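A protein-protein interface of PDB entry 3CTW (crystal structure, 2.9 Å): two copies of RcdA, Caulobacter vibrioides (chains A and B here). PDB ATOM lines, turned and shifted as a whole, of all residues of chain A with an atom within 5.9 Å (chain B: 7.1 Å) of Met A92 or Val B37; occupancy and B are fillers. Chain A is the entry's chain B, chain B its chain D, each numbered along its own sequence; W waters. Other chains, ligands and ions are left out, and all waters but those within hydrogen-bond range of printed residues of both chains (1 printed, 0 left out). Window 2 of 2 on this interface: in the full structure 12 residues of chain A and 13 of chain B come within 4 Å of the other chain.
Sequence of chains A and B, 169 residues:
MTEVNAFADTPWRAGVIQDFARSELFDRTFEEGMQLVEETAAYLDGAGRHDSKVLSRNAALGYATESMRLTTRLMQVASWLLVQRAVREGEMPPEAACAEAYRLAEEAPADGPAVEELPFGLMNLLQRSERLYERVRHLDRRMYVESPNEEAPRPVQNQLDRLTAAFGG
No position is printed for both chains.
The backbone carbonyl oxygen (O) of Ala A86 sits at hydrogen-bond distance from the backbone NH (N) of Glu A91 (2.8 Å). O of Ala A86 lies within hydrogen-bond range of N of Met A92 (3.0 Å). O of Met B75 is in hydrogen-bond range of OG of Ser B79 (2.7 Å).
Water W1 lies within hydrogen-bond range of the backbone carbonyl oxygen (O) of Thr B71 and the side-chain carboxylate (OE1) of Glu A100.
Among the printed residues, merely in contact across the chains: Glu A91 with Met B34, Met A92 with Met B34, Met A92 with Val B37, Pro A93 with Glu B38, Pro A93 with Ala B41 and Glu A100 with Met B75.
Glu A89 touches none of the printed residues of chain B. Printed residues of chain B within 4 Å of Glu A91: Met B34 (3.2 Å). Printed residues of chain B within 4 Å of Met A92: Met B34 (3.7 Å) and Val B37 (3.7 Å). Val B37 touches one residue of chain A. Of the printed residues of chain A, Glu B38 touches Pro A93 (3.9 Å). Of the printed residues of chain A, Met B75 touches Glu A100 (3.0 Å). Ala B78 touches none of the printed residues of chain A. The nearest residue of chain A that does not touch Val B37 is Ala A96 (4.1 Å).
Printed residues of chain B that touch a printed residue of chain A: Met B34, Val B37, Glu B38, Ala B41 and Met B75. Of the 13 printed residues of chain A, 4 touch a printed residue of chain B. Hydrophobic or aromatic side chains of chain A that line the printed part of chain B: Met A92 and Pro A93. Along chain A the printed residues that touch a printed residue of chain B span positions 91 to 100.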
ATOM      1  N   VAL A  83      -3.141   4.399   8.943  1.00  0.00           N
ATOM      2  CA  VAL A  83      -1.697   4.222   9.071  1.00  0.00           C
ATOM      3  C   VAL A  83      -1.012   5.556   9.357  1.00  0.00           C
ATOM      4  O   VAL A  83      -0.188   5.659  10.262  1.00  0.00           O
ATOM      5  CB  VAL A  83      -1.077   3.556   7.818  1.00  0.00           C
ATOM      6  CG1 VAL A  83       0.431   3.681   7.829  1.00  0.00           C
ATOM      7  CG2 VAL A  83      -1.469   2.094   7.748  1.00  0.00           C
ATOM      8  N   ALA A  86      -1.689   6.396  12.801  1.00  0.00           N
ATOM      9  CA  ALA A  86      -0.874   5.554  13.680  1.00  0.00           C
ATOM     10  C   ALA A  86       0.555   6.086  13.761  1.00  0.00           C
ATOM     11  O   ALA A  86       1.201   6.003  14.798  1.00  0.00           O
ATOM     12  CB  ALA A  86      -0.883   4.096  13.198  1.00  0.00           C
ATOM     13  N   VAL A  87       1.019   6.658  12.652  1.00  0.00           N
ATOM     14  CA  VAL A  87       2.321   7.302  12.582  1.00  0.00           C
ATOM     15  C   VAL A  87       2.285   8.623  13.353  1.00  0.00           C
ATOM     16  O   VAL A  87       3.240   8.973  14.041  1.00  0.00           O
ATOM     17  CB  VAL A  87       2.733   7.554  11.115  1.00  0.00           C
ATOM     18  CG1 VAL A  87       3.959   8.438  11.044  1.00  0.00           C
ATOM     19  CG2 VAL A  87       2.978   6.235  10.396  1.00  0.00           C
ATOM     20  N   ARG A  88       1.164   9.333  13.260  1.00  0.00           N
ATOM     21  CA  ARG A  88       0.987  10.595  13.976  1.00  0.00           C
ATOM     22  C   ARG A  88       0.905  10.415  15.497  1.00  0.00           C
ATOM     23  O   ARG A  88       1.283  11.317  16.245  1.00  0.00           O
ATOM     24  CB  ARG A  88      -0.241  11.353  13.460  1.00  0.00           C
ATOM     25  N   GLU A  89       0.399   9.273  15.951  1.00  0.00           N
ATOM     26  CA  GLU A  89       0.355   8.982  17.382  1.00  0.00           C
ATOM     27  C   GLU A  89       1.636   8.325  17.909  1.00  0.00           C
ATOM     28  O   GLU A  89       1.808   8.179  19.121  1.00  0.00           O
ATOM     29  CB  GLU A  89      -0.881   8.152  17.738  1.00  0.00           C
ATOM     30  CG  GLU A  89      -2.033   8.973  18.310  1.00  0.00           C
ATOM     31  CD  GLU A  89      -2.522  10.066  17.370  1.00  0.00           C
ATOM     32  OE1 GLU A  89      -2.643   9.804  16.150  1.00  0.00           O
ATOM     33  OE2 GLU A  89      -2.794  11.187  17.855  1.00  0.00           O
ATOM     34  N   GLY A  90       2.532   7.937  17.003  1.00  0.00           N
ATOM     35  CA  GLY A  90       3.778   7.273  17.392  1.00  0.00           C
ATOM     36  C   GLY A  90       3.654   5.764  17.553  1.00  0.00           C
ATOM     37  O   GLY A  90       4.568   5.100  18.047  1.00  0.00           O
ATOM     38  N   GLU A  91       2.520   5.216  17.130  1.00  0.00           N
ATOM     39  CA  GLU A  91       2.325   3.773  17.112  1.00  0.00           C
ATOM     40  C   GLU A  91       3.121   3.118  15.989  1.00  0.00           C
ATOM     41  O   GLU A  91       3.545   1.963  16.100  1.00  0.00           O
ATOM     42  CB  GLU A  91       0.844   3.442  16.990  1.00  0.00           C
ATOM     43  CG  GLU A  91       0.077   3.744  18.263  1.00  0.00           C
ATOM     44  CD  GLU A  91      -1.423   3.880  18.053  1.00  0.00           C
ATOM     45  OE1 GLU A  91      -2.151   3.934  19.070  1.00  0.00           O
ATOM     46  OE2 GLU A  91      -1.876   3.939  16.887  1.00  0.00           O
ATOM     47  N   MET A  92       3.318   3.859  14.907  1.00  0.00           N
ATOM     48  CA  MET A  92       4.131   3.400  13.794  1.00  0.00           C
ATOM     49  C   MET A  92       5.229   4.398  13.470  1.00  0.00           C
ATOM     50  O   MET A  92       5.018   5.608  13.581  1.00  0.00           O
ATOM     51  CB  MET A  92       3.252   3.182  12.577  1.00  0.00           C
ATOM     52  CG  MET A  92       2.466   1.894  12.642  1.00  0.00           C
ATOM     53  SD  MET A  92       1.565   1.617  11.131  1.00  0.00           S
ATOM     54  CE  MET A  92       2.889   1.259   9.962  1.00  0.00           C
ATOM     55  N   PRO A  93       6.409   3.898  13.073  1.00  0.00           N
ATOM     56  CA  PRO A  93       7.537   4.780  12.807  1.00  0.00           C
ATOM     57  C   PRO A  93       7.309   5.599  11.540  1.00  0.00           C
ATOM     58  O   PRO A  93       6.704   5.099  10.589  1.00  0.00           O
ATOM     59  CB  PRO A  93       8.714   3.810  12.630  1.00  0.00           C
ATOM     60  CG  PRO A  93       8.274   2.562  13.276  1.00  0.00           C
ATOM     61  CD  PRO A  93       6.808   2.488  12.987  1.00  0.00           C
ATOM     62  N   PRO A  94       7.785   6.856  11.532  1.00  0.00           N
ATOM     63  CA  PRO A  94       7.627   7.756  10.395  1.00  0.00           C
ATOM     64  C   PRO A  94       8.296   7.209   9.138  1.00  0.00           C
ATOM     65  O   PRO A  94       7.971   7.621   8.026  1.00  0.00           O
ATOM     66  CB  PRO A  94       8.349   9.029  10.856  1.00  0.00           C
ATOM     67  CG  PRO A  94       9.274   8.586  11.953  1.00  0.00           C
ATOM     68  CD  PRO A  94       8.535   7.488  12.635  1.00  0.00           C
ATOM     69  N   ALA A  96       8.285   3.998   8.348  1.00  0.00           N
ATOM     70  CA  ALA A  96       7.504   2.898   7.831  1.00  0.00           C
ATOM     71  C   ALA A  96       6.318   3.505   7.209  1.00  0.00           C
ATOM     72  O   ALA A  96       5.489   4.049   7.886  1.00  0.00           O
ATOM     73  CB  ALA A  96       7.084   2.029   8.911  1.00  0.00           C
ATOM     74  N   ALA A  97       6.202   3.334   5.903  1.00  0.00           N
ATOM     75  CA  ALA A  97       5.100   3.893   5.147  1.00  0.00           C
ATOM     76  C   ALA A  97       5.744   4.432   3.893  1.00  0.00           C
ATOM     77  O   ALA A  97       5.079   4.993   3.022  1.00  0.00           O
ATOM     78  CB  ALA A  97       4.436   5.016   5.930  1.00  0.00           C
ATOM     79  N   GLU A 100       4.546   1.964   1.274  1.00  0.00           N
ATOM     80  CA  GLU A 100       3.242   1.564   1.767  1.00  0.00           C
ATOM     81  C   GLU A 100       2.192   2.087   0.851  1.00  0.00           C
ATOM     82  O   GLU A 100       1.735   3.206   0.998  1.00  0.00           O
ATOM     83  CB  GLU A 100       3.036   2.043   3.193  1.00  0.00           C
ATOM     84  CG  GLU A 100       3.973   1.346   4.159  1.00  0.00           C
ATOM     85  CD  GLU A 100       3.257   0.724   5.304  1.00  0.00           C
ATOM     86  OE1 GLU A 100       3.807  -0.125   6.016  1.00  0.00           O
ATOM     87  OE2 GLU A 100       2.116   1.101   5.500  1.00  0.00           O
ATOM     88  N   GLU B  32       2.052  -7.594  18.521  1.00  0.00           N
ATOM     89  CA  GLU B  32       3.079  -8.340  17.790  1.00  0.00           C
ATOM     90  C   GLU B  32       3.302  -7.706  16.428  1.00  0.00           C
ATOM     91  O   GLU B  32       4.440  -7.619  15.958  1.00  0.00           O
ATOM     92  CB  GLU B  32       2.696  -9.829  17.631  1.00  0.00           C
ATOM     93  CG  GLU B  32       3.647 -10.669  16.746  1.00  0.00           C
ATOM     94  CD  GLU B  32       3.207 -12.120  16.570  1.00  0.00           C
ATOM     95  OE1 GLU B  32       2.539 -12.665  17.471  1.00  0.00           O
ATOM     96  OE2 GLU B  32       3.542 -12.725  15.530  1.00  0.00           O
ATOM     97  N   GLY B  33       2.209  -7.258  15.815  1.00  0.00           N
ATOM     98  CA  GLY B  33       2.248  -6.636  14.497  1.00  0.00           C
ATOM     99  C   GLY B  33       2.939  -5.291  14.498  1.00  0.00           C
ATOM    100  O   GLY B  33       3.766  -5.004  13.636  1.00  0.00           O
ATOM    101  N   MET B  34       2.615  -4.489  15.504  1.00  0.00           N
ATOM    102  CA  MET B  34       3.135  -3.143  15.646  1.00  0.00           C
ATOM    103  C   MET B  34       4.618  -3.138  16.029  1.00  0.00           C
ATOM    104  O   MET B  34       5.365  -2.250  15.620  1.00  0.00           O
ATOM    105  CB  MET B  34       2.300  -2.388  16.683  1.00  0.00           C
ATOM    106  CG  MET B  34       0.813  -2.283  16.334  1.00  0.00           C
ATOM    107  SD  MET B  34       0.526  -1.257  14.860  1.00  0.00           S
ATOM    108  CE  MET B  34       0.784   0.379  15.528  1.00  0.00           C
ATOM    109  N   GLN B  35       5.041  -4.152  16.782  1.00  0.00           N
ATOM    110  CA  GLN B  35       6.449  -4.296  17.177  1.00  0.00           C
ATOM    111  C   GLN B  35       7.339  -4.742  16.001  1.00  0.00           C
ATOM    112  O   GLN B  35       8.454  -4.246  15.817  1.00  0.00           O
ATOM    113  CB  GLN B  35       6.578  -5.272  18.348  1.00  0.00           C
ATOM    114  CG  GLN B  35       8.007  -5.397  18.857  1.00  0.00           C
ATOM    115  CD  GLN B  35       8.147  -6.295  20.058  1.00  0.00           C
ATOM    116  OE1 GLN B  35       9.087  -7.082  20.155  1.00  0.00           O
ATOM    117  NE2 GLN B  35       7.220  -6.174  20.990  1.00  0.00           N
ATOM    118  N   LEU B  36       6.819  -5.660  15.194  1.00  0.00           N
ATOM    119  CA  LEU B  36       7.557  -6.174  14.051  1.00  0.00           C
ATOM    120  C   LEU B  36       7.751  -5.088  13.004  1.00  0.00           C
ATOM    121  O   LEU B  36       8.817  -5.000  12.388  1.00  0.00           O
ATOM    122  CB  LEU B  36       6.821  -7.354  13.439  1.00  0.00           C
ATOM    123  CG  LEU B  36       7.645  -8.483  12.827  1.00  0.00           C
ATOM    124  CD1 LEU B  36       6.698  -9.641  12.592  1.00  0.00           C
ATOM    125  CD2 LEU B  36       8.340  -8.086  11.527  1.00  0.00           C
ATOM    126  N   VAL B  37       6.723  -4.255  12.815  1.00  0.00           N
ATOM    127  CA  VAL B  37       6.812  -3.091  11.950  1.00  0.00           C
ATOM    128  C   VAL B  37       7.882  -2.135  12.460  1.00  0.00           C
ATOM    129  O   VAL B  37       8.635  -1.564  11.674  1.00  0.00           O
ATOM    130  CB  VAL B  37       5.437  -2.367  11.820  1.00  0.00           C
ATOM    131  CG1 VAL B  37       5.591  -1.018  11.130  1.00  0.00           C
ATOM    132  CG2 VAL B  37       4.462  -3.238  11.057  1.00  0.00           C
ATOM    133  N   GLU B  38       7.959  -1.994  13.779  1.00  0.00           N
ATOM    134  CA  GLU B  38       8.905  -1.077  14.405  1.00  0.00           C
ATOM    135  C   GLU B  38      10.336  -1.597  14.281  1.00  0.00           C
ATOM    136  O   GLU B  38      11.262  -0.835  14.004  1.00  0.00           O
ATOM    137  CB  GLU B  38       8.539  -0.860  15.879  1.00  0.00           C
ATOM    138  CG  GLU B  38       9.349   0.231  16.560  1.00  0.00           C
ATOM    139  CD  GLU B  38       9.116   0.291  18.060  1.00  0.00           C
ATOM    140  OE1 GLU B  38       8.844  -0.778  18.663  1.00  0.00           O
ATOM    141  OE2 GLU B  38       9.207   1.404  18.634  1.00  0.00           O
ATOM    142  N   GLU B  39      10.498  -2.904  14.464  1.00  0.00           N
ATOM    143  CA  GLU B  39      11.808  -3.543  14.381  1.00  0.00           C
ATOM    144  C   GLU B  39      12.335  -3.592  12.949  1.00  0.00           C
ATOM    145  O   GLU B  39      13.539  -3.503  12.725  1.00  0.00           O
ATOM    146  CB  GLU B  39      11.783  -4.949  15.000  1.00  0.00           C
ATOM    147  CG  GLU B  39      11.633  -4.936  16.502  1.00  0.00           C
ATOM    148  CD  GLU B  39      11.865  -6.291  17.116  1.00  0.00           C
ATOM    149  OE1 GLU B  39      12.908  -6.908  16.794  1.00  0.00           O
ATOM    150  OE2 GLU B  39      11.004  -6.754  17.899  1.00  0.00           O
ATOM    151  N   THR B  40      11.420  -3.721  11.996  1.00  0.00           N
ATOM    152  CA  THR B  40      11.760  -3.754  10.581  1.00  0.00           C
ATOM    153  C   THR B  40      12.257  -2.393  10.125  1.00  0.00           C
ATOM    154  O   THR B  40      13.253  -2.291   9.403  1.00  0.00           O
ATOM    155  CB  THR B  40      10.540  -4.186   9.736  1.00  0.00           C
ATOM    156  OG1 THR B  40      10.154  -5.506  10.134  1.00  0.00           O
ATOM    157  CG2 THR B  40      10.859  -4.166   8.257  1.00  0.00           C
ATOM    158  N   ALA B  41      11.573  -1.351  10.586  1.00  0.00           N
ATOM    159  CA  ALA B  41      11.904   0.007  10.232  1.00  0.00           C
ATOM    160  C   ALA B  41      13.218   0.408  10.880  1.00  0.00           C
ATOM    161  O   ALA B  41      13.958   1.191  10.318  1.00  0.00           O
ATOM    162  CB  ALA B  41      10.788   0.938  10.657  1.00  0.00           C
ATOM    163  N   ALA B  42      13.517  -0.153  12.051  1.00  0.00           N
ATOM    164  CA  ALA B  42      14.771   0.113  12.744  1.00  0.00           C
ATOM    165  C   ALA B  42      15.931  -0.629  12.084  1.00  0.00           C
ATOM    166  O   ALA B  42      17.060  -0.142  12.066  1.00  0.00           O
ATOM    167  CB  ALA B  42      14.651  -0.268  14.214  1.00  0.00           C
ATOM    168  N   TYR B  43      15.629  -1.790  11.513  1.00  0.00           N
ATOM    169  CA  TYR B  43      16.641  -2.643  10.907  1.00  0.00           C
ATOM    170  C   TYR B  43      17.008  -2.187   9.502  1.00  0.00           C
ATOM    171  O   TYR B  43      18.184  -1.957   9.212  1.00  0.00           O
ATOM    172  CB  TYR B  43      16.168  -4.106  10.878  1.00  0.00           C
ATOM    173  CG  TYR B  43      17.081  -5.041  10.110  1.00  0.00           C
ATOM    174  CD1 TYR B  43      18.277  -5.501  10.662  1.00  0.00           C
ATOM    175  CD2 TYR B  43      16.752  -5.451   8.825  1.00  0.00           C
ATOM    176  CE1 TYR B  43      19.110  -6.348   9.956  1.00  0.00           C
ATOM    177  CE2 TYR B  43      17.586  -6.298   8.110  1.00  0.00           C
ATOM    178  CZ  TYR B  43      18.762  -6.739   8.678  1.00  0.00           C
ATOM    179  OH  TYR B  43      19.584  -7.576   7.964  1.00  0.00           O
ATOM    180  N   THR B  71       8.144  -5.755   3.739  1.00  0.00           N
ATOM    181  CA  THR B  71       7.526  -4.497   4.112  1.00  0.00           C
ATOM    182  C   THR B  71       6.101  -4.343   3.565  1.00  0.00           C
ATOM    183  O   THR B  71       5.248  -3.741   4.202  1.00  0.00           O
ATOM    184  CB  THR B  71       8.433  -3.299   3.736  1.00  0.00           C
ATOM    185  OG1 THR B  71       7.910  -2.115   4.339  1.00  0.00           O
ATOM    186  CG2 THR B  71       8.517  -3.104   2.227  1.00  0.00           C
ATOM    187  N   LEU B  74       3.920  -6.528   5.799  1.00  0.00           N
ATOM    188  CA  LEU B  74       3.669  -5.948   7.108  1.00  0.00           C
ATOM    189  C   LEU B  74       2.633  -4.830   7.045  1.00  0.00           C
ATOM    190  O   LEU B  74       1.850  -4.636   7.992  1.00  0.00           O
ATOM    191  CB  LEU B  74       4.958  -5.431   7.728  1.00  0.00           C
ATOM    192  CG  LEU B  74       6.002  -6.443   8.218  1.00  0.00           C
ATOM    193  CD1 LEU B  74       7.224  -5.681   8.708  1.00  0.00           C
ATOM    194  CD2 LEU B  74       5.457  -7.360   9.306  1.00  0.00           C
ATOM    195  N   MET B  75       2.618  -4.091   5.936  1.00  0.00           N
ATOM    196  CA  MET B  75       1.619  -3.040   5.756  1.00  0.00           C
ATOM    197  C   MET B  75       0.243  -3.640   5.515  1.00  0.00           C
ATOM    198  O   MET B  75      -0.777  -3.024   5.808  1.00  0.00           O
ATOM    199  CB  MET B  75       2.010  -2.099   4.617  1.00  0.00           C
ATOM    200  CG  MET B  75       1.897  -2.678   3.205  1.00  0.00           C
ATOM    201  SD  MET B  75       0.167  -2.701   2.581  1.00  0.00           S
ATOM    202  CE  MET B  75      -0.329  -0.993   2.678  1.00  0.00           C
ATOM    203  N   VAL B  77      -0.744  -6.379   7.016  1.00  0.00           N
ATOM    204  CA  VAL B  77      -1.187  -6.810   8.329  1.00  0.00           C
ATOM    205  C   VAL B  77      -1.476  -5.606   9.220  1.00  0.00           C
ATOM    206  O   VAL B  77      -2.500  -5.561   9.904  1.00  0.00           O
ATOM    207  CB  VAL B  77      -0.130  -7.723   9.001  1.00  0.00           C
ATOM    208  CG1 VAL B  77      -0.568  -8.128  10.406  1.00  0.00           C
ATOM    209  CG2 VAL B  77       0.112  -8.958   8.164  1.00  0.00           C
ATOM    210  N   ALA B  78      -0.569  -4.627   9.200  1.00  0.00           N
ATOM    211  CA  ALA B  78      -0.738  -3.381   9.945  1.00  0.00           C
ATOM    212  C   ALA B  78      -2.061  -2.690   9.579  1.00  0.00           C
ATOM    213  O   ALA B  78      -2.810  -2.243  10.455  1.00  0.00           O
ATOM    214  CB  ALA B  78       0.455  -2.452   9.699  1.00  0.00           C
ATOM    215  N   SER B  79      -2.363  -2.659   8.282  1.00  0.00           N
ATOM    216  CA  SER B  79      -3.602  -2.073   7.794  1.00  0.00           C
ATOM    217  C   SER B  79      -4.805  -2.882   8.266  1.00  0.00           C
ATOM    218  O   SER B  79      -5.810  -2.313   8.653  1.00  0.00           O
ATOM    219  CB  SER B  79      -3.594  -1.974   6.272  1.00  0.00           C
ATOM    220  OG  SER B  79      -3.476  -3.256   5.696  1.00  0.00           O
ATOM    221  N   LEU B  81      -4.866  -4.921  11.049  1.00  0.00           N
ATOM    222  CA  LEU B  81      -4.936  -4.760  12.493  1.00  0.00           C
ATOM    223  C   LEU B  81      -5.710  -3.516  12.881  1.00  0.00           C
ATOM    224  O   LEU B  81      -6.588  -3.563  13.733  1.00  0.00           O
ATOM    225  CB  LEU B  81      -3.535  -4.727  13.106  1.00  0.00           C
ATOM    226  CG  LEU B  81      -2.873  -6.111  13.218  1.00  0.00           C
ATOM    227  CD1 LEU B  81      -1.442  -6.044  13.769  1.00  0.00           C
ATOM    228  CD2 LEU B  81      -3.735  -6.981  14.095  1.00  0.00           C
ATOM    229  N   LEU B  82      -5.391  -2.399  12.246  1.00  0.00           N
ATOM    230  CA  LEU B  82      -6.014  -1.130  12.593  1.00  0.00           C
ATOM    231  C   LEU B  82      -7.459  -1.054  12.162  1.00  0.00           C
ATOM    232  O   LEU B  82      -8.172  -0.141  12.530  1.00  0.00           O
ATOM    233  CB  LEU B  82      -5.265   0.010  11.907  1.00  0.00           C
ATOM    234  CG  LEU B  82      -3.874   0.305  12.468  1.00  0.00           C
ATOM    235  CD1 LEU B  82      -3.068   1.136  11.498  1.00  0.00           C
ATOM    236  CD2 LEU B  82      -3.970   0.980  13.860  1.00  0.00           C
ATOM    237  N   LEU B 125      13.206 -11.352  10.631  1.00  0.00           N
ATOM    238  CA  LEU B 125      12.033 -10.530  10.385  1.00  0.00           C
ATOM    239  C   LEU B 125      11.095 -11.165   9.370  1.00  0.00           C
ATOM    240  O   LEU B 125       9.873 -11.062   9.502  1.00  0.00           O
ATOM    241  CB  LEU B 125      12.454  -9.157   9.884  1.00  0.00           C
ATOM    242  CG  LEU B 125      13.154  -8.200  10.845  1.00  0.00           C
ATOM    243  CD1 LEU B 125      13.753  -7.088  10.056  1.00  0.00           C
ATOM    244  CD2 LEU B 125      12.184  -7.663  11.863  1.00  0.00           C
ATOM    245  N   LEU B 132       3.303 -14.134  11.587  1.00  0.00           N
ATOM    246  CA  LEU B 132       2.321 -13.098  11.905  1.00  0.00           C
ATOM    247  C   LEU B 132       1.191 -13.098  10.875  1.00  0.00           C
ATOM    248  O   LEU B 132       0.022 -12.897  11.208  1.00  0.00           O
ATOM    249  CB  LEU B 132       3.009 -11.738  11.897  1.00  0.00           C
ATOM    250  CG  LEU B 132       2.547 -10.569  12.771  1.00  0.00           C
ATOM    251  CD1 LEU B 132       3.152  -9.271  12.223  1.00  0.00           C
ATOM    252  CD2 LEU B 132       1.048 -10.430  12.892  1.00  0.00           C
HETATM  253  O   HOH W   1       6.052  -2.352   6.826  1.00  0.00           O
